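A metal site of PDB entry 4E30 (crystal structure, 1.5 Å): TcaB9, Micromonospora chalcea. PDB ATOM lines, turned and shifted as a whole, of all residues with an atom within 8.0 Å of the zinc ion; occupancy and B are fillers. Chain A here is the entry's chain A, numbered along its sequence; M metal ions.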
ATOM      1  N   ALA A  14      12.091  -8.110  22.477  1.00  0.00           N
ATOM      2  CA  ALA A  14      10.955  -7.215  22.744  1.00  0.00           C
ATOM      3  C   ALA A  14       9.626  -7.931  22.429  1.00  0.00           C
ATOM      4  O   ALA A  14       9.496  -8.552  21.367  1.00  0.00           O
ATOM      5  CB  ALA A  14      11.073  -5.906  21.948  1.00  0.00           C
ATOM      6  N   CYS A  15       8.660  -7.837  23.332  1.00  0.00           N
ATOM      7  CA  CYS A  15       7.298  -8.301  23.099  1.00  0.00           C
ATOM      8  C   CYS A  15       6.735  -7.736  21.796  1.00  0.00           C
ATOM      9  O   CYS A  15       6.750  -6.510  21.578  1.00  0.00           O
ATOM     10  CB  CYS A  15       6.390  -7.956  24.268  1.00  0.00           C
ATOM     11  SG  CYS A  15       4.669  -8.484  24.031  1.00  0.00           S
ATOM     12  N   ARG A  16       6.219  -8.632  20.950  1.00  0.00           N
ATOM     13  CA  ARG A  16       5.577  -8.243  19.708  1.00  0.00           C
ATOM     14  C   ARG A  16       4.217  -7.561  19.846  1.00  0.00           C
ATOM     15  O   ARG A  16       3.735  -6.939  18.886  1.00  0.00           O
ATOM     16  CB  ARG A  16       5.487  -9.411  18.717  1.00  0.00           C
ATOM     17  CG  ARG A  16       6.773  -9.670  17.989  1.00  0.00           C
ATOM     18  CD  ARG A  16       7.200  -8.452  17.109  1.00  0.00           C
ATOM     19  NE  ARG A  16       7.487  -8.919  15.760  1.00  0.00           N
ATOM     20  CZ  ARG A  16       7.106  -8.357  14.619  1.00  0.00           C
ATOM     21  NH1 ARG A  16       7.483  -8.938  13.497  1.00  0.00           N
ATOM     22  NH2 ARG A  16       6.370  -7.243  14.557  1.00  0.00           N
ATOM     23  N   VAL A  17       3.618  -7.654  21.035  1.00  0.00           N
ATOM     24  CA  VAL A  17       2.343  -6.982  21.229  1.00  0.00           C
ATOM     25  C   VAL A  17       2.559  -5.587  21.839  1.00  0.00           C
ATOM     26  O   VAL A  17       1.953  -4.635  21.352  1.00  0.00           O
ATOM     27  CB  VAL A  17       1.403  -7.798  22.141  1.00  0.00           C
ATOM     28  CG1 VAL A  17       0.190  -6.978  22.514  1.00  0.00           C
ATOM     29  CG2 VAL A  17       0.961  -9.016  21.378  1.00  0.00           C
ATOM     30  N   CYS A  18       3.388  -5.486  22.877  1.00  0.00           N
ATOM     31  CA  CYS A  18       3.441  -4.216  23.602  1.00  0.00           C
ATOM     32  C   CYS A  18       4.860  -3.671  23.721  1.00  0.00           C
ATOM     33  O   CYS A  18       4.996  -2.560  24.241  1.00  0.00           O
ATOM     34  CB  CYS A  18       2.864  -4.309  25.020  1.00  0.00           C
ATOM     35  SG  CYS A  18       3.853  -5.304  26.143  1.00  0.00           S
ATOM     36  N   GLY A  19       5.873  -4.399  23.281  1.00  0.00           N
ATOM     37  CA  GLY A  19       7.273  -3.945  23.410  1.00  0.00           C
ATOM     38  C   GLY A  19       7.857  -4.097  24.808  1.00  0.00           C
ATOM     39  O   GLY A  19       9.020  -3.729  25.044  1.00  0.00           O
ATOM     40  N   GLY A  20       7.105  -4.654  25.751  1.00  0.00           N
ATOM     41  CA  GLY A  20       7.625  -5.094  27.036  1.00  0.00           C
ATOM     42  C   GLY A  20       8.809  -6.047  26.921  1.00  0.00           C
ATOM     43  O   GLY A  20       9.195  -6.459  25.822  1.00  0.00           O
ATOM     44  N   GLY A  21       9.404  -6.445  28.041  1.00  0.00           N
ATOM     45  CA  GLY A  21      10.490  -7.421  27.965  1.00  0.00           C
ATOM     46  C   GLY A  21       9.969  -8.844  28.048  1.00  0.00           C
ATOM     47  O   GLY A  21       9.047  -9.121  28.844  1.00  0.00           O
ATOM     48  N   VAL A  22      10.576  -9.721  27.254  1.00  0.00           N
ATOM     49  CA  VAL A  22      10.186 -11.126  27.272  1.00  0.00           C
ATOM     50  C   VAL A  22      11.122 -12.000  28.078  1.00  0.00           C
ATOM     51  O   VAL A  22      12.326 -12.009  27.779  1.00  0.00           O
ATOM     52  CB  VAL A  22      10.047 -11.733  25.855  1.00  0.00           C
ATOM     53  CG1 VAL A  22       9.708 -13.209  25.868  1.00  0.00           C
ATOM     54  CG2 VAL A  22       9.009 -10.902  25.096  1.00  0.00           C
ATOM     55  N   ARG A  55       7.680 -15.104  28.160  1.00  0.00           N
ATOM     56  CA  ARG A  55       6.429 -14.431  28.513  1.00  0.00           C
ATOM     57  C   ARG A  55       6.743 -12.958  28.641  1.00  0.00           C
ATOM     58  O   ARG A  55       7.759 -12.611  29.278  1.00  0.00           O
ATOM     59  CB  ARG A  55       5.811 -14.963  29.818  1.00  0.00           C
ATOM     60  CG  ARG A  55       4.447 -14.319  30.022  1.00  0.00           C
ATOM     61  CD  ARG A  55       4.022 -14.243  31.487  1.00  0.00           C
ATOM     62  NE  ARG A  55       4.794 -13.187  32.132  1.00  0.00           N
ATOM     63  CZ  ARG A  55       4.842 -12.946  33.438  1.00  0.00           C
ATOM     64  NH1 ARG A  55       5.622 -11.952  33.860  1.00  0.00           N
ATOM     65  NH2 ARG A  55       4.171 -13.695  34.306  1.00  0.00           N
ATOM     66  N   CYS A  56       5.914 -12.090  28.066  1.00  0.00           N
ATOM     67  CA  CYS A  56       6.179 -10.674  28.203  1.00  0.00           C
ATOM     68  C   CYS A  56       5.949 -10.257  29.673  1.00  0.00           C
ATOM     69  O   CYS A  56       4.974 -10.695  30.298  1.00  0.00           O
ATOM     70  CB  CYS A  56       5.200  -9.894  27.319  1.00  0.00           C
ATOM     71  SG  CYS A  56       5.299  -8.101  27.597  1.00  0.00           S
ATOM     72  N   ASP A  57       6.807  -9.357  30.160  1.00  0.00           N
ATOM     73  CA  ASP A  57       6.677  -8.728  31.481  1.00  0.00           C
ATOM     74  C   ASP A  57       5.448  -7.848  31.708  1.00  0.00           C
ATOM     75  O   ASP A  57       4.948  -7.728  32.836  1.00  0.00           O
ATOM     76  CB  ASP A  57       7.868  -7.794  31.702  1.00  0.00           C
ATOM     77  CG  ASP A  57       9.114  -8.553  32.051  1.00  0.00           C
ATOM     78  OD1 ASP A  57       8.921  -9.640  32.647  1.00  0.00           O
ATOM     79  OD2 ASP A  57      10.217  -8.076  31.709  1.00  0.00           O
ATOM     80  N   SER A  58       4.979  -7.224  30.643  1.00  0.00           N
ATOM     81  CA  SER A  58       3.957  -6.199  30.740  1.00  0.00           C
ATOM     82  C   SER A  58       2.560  -6.693  30.389  1.00  0.00           C
ATOM     83  O   SER A  58       1.613  -6.368  31.098  1.00  0.00           O
ATOM     84  CB  SER A  58       4.324  -5.041  29.817  1.00  0.00           C
ATOM     85  OG  SER A  58       5.556  -4.505  30.252  1.00  0.00           O
ATOM     86  N   CYS A  59       2.412  -7.454  29.312  1.00  0.00           N
ATOM     87  CA  CYS A  59       1.085  -7.896  28.887  1.00  0.00           C
ATOM     88  C   CYS A  59       0.739  -9.378  29.066  1.00  0.00           C
ATOM     89  O   CYS A  59      -0.373  -9.817  28.756  1.00  0.00           O
ATOM     90  CB  CYS A  59       0.835  -7.435  27.461  1.00  0.00           C
ATOM     91  SG  CYS A  59       1.702  -8.524  26.275  1.00  0.00           S
ATOM     92  N   GLU A  60       1.714 -10.144  29.554  1.00  0.00           N
ATOM     93  CA  GLU A  60       1.518 -11.578  29.791  1.00  0.00           C
ATOM     94  C   GLU A  60       1.415 -12.492  28.578  1.00  0.00           C
ATOM     95  O   GLU A  60       1.114 -13.675  28.737  1.00  0.00           O
ATOM     96  CB  GLU A  60       0.420 -11.974  30.770  1.00  0.00           C
ATOM     97  CG  GLU A  60       0.754 -11.265  32.101  1.00  0.00           C
ATOM     98  CD  GLU A  60      -0.256 -11.601  33.170  1.00  0.00           C
ATOM     99  OE1 GLU A  60      -0.186 -12.752  33.634  1.00  0.00           O
ATOM    100  OE2 GLU A  60      -1.099 -10.733  33.499  1.00  0.00           O
ATOM    101  N   MET A  61       1.667 -11.904  27.411  1.00  0.00           N
ATOM    102  CA  MET A  61       1.730 -12.707  26.203  1.00  0.00           C
ATOM    103  C   MET A  61       2.905 -13.674  26.173  1.00  0.00           C
ATOM    104  O   MET A  61       4.086 -13.303  26.262  1.00  0.00           O
ATOM    105  CB  MET A  61       1.774 -11.835  24.958  1.00  0.00           C
ATOM    106  CG  MET A  61       1.685 -12.571  23.618  1.00  0.00           C
ATOM    107  SD  MET A  61       0.113 -13.439  23.433  1.00  0.00           S
ATOM    108  CE  MET A  61      -0.970 -12.079  22.975  1.00  0.00           C
ATOM    109  N   VAL A  62       2.552 -14.938  25.971  1.00  0.00           N
ATOM    110  CA  VAL A  62       3.599 -15.968  25.839  1.00  0.00           C
ATOM    111  C   VAL A  62       3.873 -16.059  24.345  1.00  0.00           C
ATOM    112  O   VAL A  62       2.970 -16.183  23.504  1.00  0.00           O
ATOM    113  CB  VAL A  62       2.965 -17.268  26.368  1.00  0.00           C
ATOM    114  CG1 VAL A  62       3.817 -18.479  26.009  1.00  0.00           C
ATOM    115  CG2 VAL A  62       2.792 -17.157  27.925  1.00  0.00           C
ATOM    116  N   GLN A  63       5.171 -16.026  23.993  1.00  0.00           N
ATOM    117  CA  GLN A  63       5.585 -15.973  22.603  1.00  0.00           C
ATOM    118  C   GLN A  63       6.976 -16.559  22.436  1.00  0.00           C
ATOM    119  O   GLN A  63       7.731 -16.623  23.403  1.00  0.00           O
ATOM    120  CB  GLN A  63       5.624 -14.540  22.101  1.00  0.00           C
ATOM    121  CG  GLN A  63       6.573 -13.634  22.892  1.00  0.00           C
ATOM    122  CD  GLN A  63       6.094 -12.221  22.791  1.00  0.00           C
ATOM    123  OE1 GLN A  63       6.395 -11.500  21.842  1.00  0.00           O
ATOM    124  NE2 GLN A  63       5.301 -11.809  23.768  1.00  0.00           N
ATOM    125  N   PHE A 229       2.658 -17.474  19.035  1.00  0.00           N
ATOM    126  CA  PHE A 229       1.993 -17.068  20.284  1.00  0.00           C
ATOM    127  C   PHE A 229       1.243 -18.250  20.831  1.00  0.00           C
ATOM    128  O   PHE A 229       0.618 -19.002  20.074  1.00  0.00           O
ATOM    129  CB  PHE A 229       0.929 -15.978  19.994  1.00  0.00           C
ATOM    130  CG  PHE A 229       1.524 -14.647  19.599  1.00  0.00           C
ATOM    131  CD1 PHE A 229       2.303 -13.926  20.493  1.00  0.00           C
ATOM    132  CD2 PHE A 229       1.289 -14.148  18.301  1.00  0.00           C
ATOM    133  CE1 PHE A 229       2.864 -12.703  20.101  1.00  0.00           C
ATOM    134  CE2 PHE A 229       1.816 -12.907  17.934  1.00  0.00           C
ATOM    135  CZ  PHE A 229       2.578 -12.157  18.829  1.00  0.00           C
ATOM    136  N   SER A 235      -3.926 -12.575  27.987  1.00  0.00           N
ATOM    137  CA  SER A 235      -3.124 -11.817  27.001  1.00  0.00           C
ATOM    138  C   SER A 235      -3.919 -11.316  25.795  1.00  0.00           C
ATOM    139  O   SER A 235      -3.609 -10.249  25.281  1.00  0.00           O
ATOM    140  CB  SER A 235      -1.949 -12.695  26.556  1.00  0.00           C
ATOM    141  OG  SER A 235      -2.327 -13.850  25.812  1.00  0.00           O
ATOM    142  N   MET A 239      -4.076  -7.564  24.507  1.00  0.00           N
ATOM    143  CA  MET A 239      -3.733  -7.221  23.140  1.00  0.00           C
ATOM    144  C   MET A 239      -4.845  -6.448  22.461  1.00  0.00           C
ATOM    145  O   MET A 239      -4.640  -5.471  21.733  1.00  0.00           O
ATOM    146  CB  MET A 239      -3.418  -8.529  22.409  1.00  0.00           C
ATOM    147  CG  MET A 239      -3.221  -8.351  20.900  1.00  0.00           C
ATOM    148  SD  MET A 239      -2.812  -9.939  20.128  1.00  0.00           S
ATOM    149  CE  MET A 239      -4.407 -10.777  20.072  1.00  0.00           C
ATOM    150  N   ARG A 242      -5.150  -2.842  23.839  1.00  0.00           N
ATOM    151  CA  ARG A 242      -4.070  -1.949  23.408  1.00  0.00           C
ATOM    152  C   ARG A 242      -4.270  -1.474  21.980  1.00  0.00           C
ATOM    153  O   ARG A 242      -3.637  -0.505  21.570  1.00  0.00           O
ATOM    154  CB  ARG A 242      -2.709  -2.631  23.545  1.00  0.00           C
ATOM    155  CG  ARG A 242      -2.231  -2.780  24.970  1.00  0.00           C
ATOM    156  CD  ARG A 242      -1.096  -3.813  24.975  1.00  0.00           C
ATOM    157  NE  ARG A 242      -0.320  -3.580  26.182  1.00  0.00           N
ATOM    158  CZ  ARG A 242      -0.531  -4.165  27.360  1.00  0.00           C
ATOM    159  NH1 ARG A 242      -1.527  -5.036  27.512  1.00  0.00           N
ATOM    160  NH2 ARG A 242       0.257  -3.860  28.377  1.00  0.00           N
HETATM  161 ZN    ZN M   1       3.699  -7.520  25.872  1.00  0.00          ZN
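N of Gly 20 lies close to SG of Cys 18, at 3.3 Å.
The side-chain sulfur (SG) of Cys 59 sits close to the backbone NH (N) of Met 61 (3.6 Å).
The backbone NH of Val 17 lies close to the side-chain sulfur of Cys 15 (3.3 Å).
The backbone NH (N) of Cys 15 sits at hydrogen-bond distance from the backbone carbonyl oxygen (O) of Gly 20, at 2.9 Å.
The side-chain amide nitrogen (NE2) of Gln 63 sits close to the side-chain sulfur (SG) of Cys 15 (3.4 Å).
N of Ser 58 sits close to SG of Cys 56, at 3.2 Å.
O of Met 61 is in hydrogen-bond range of N of Cys 56, at 2.8 Å.
The zinc ion is bound by the side-chain sulfur (SG) of Cys 18, the side-chain sulfur (SG) of Cys 59, the side-chain sulfur (SG) of Cys 15 and the side-chain sulfur (SG) of Cys 56.
Within 4 Å of the zinc ion: Cys 15, Cys 18, Cys 56 and Cys 59.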
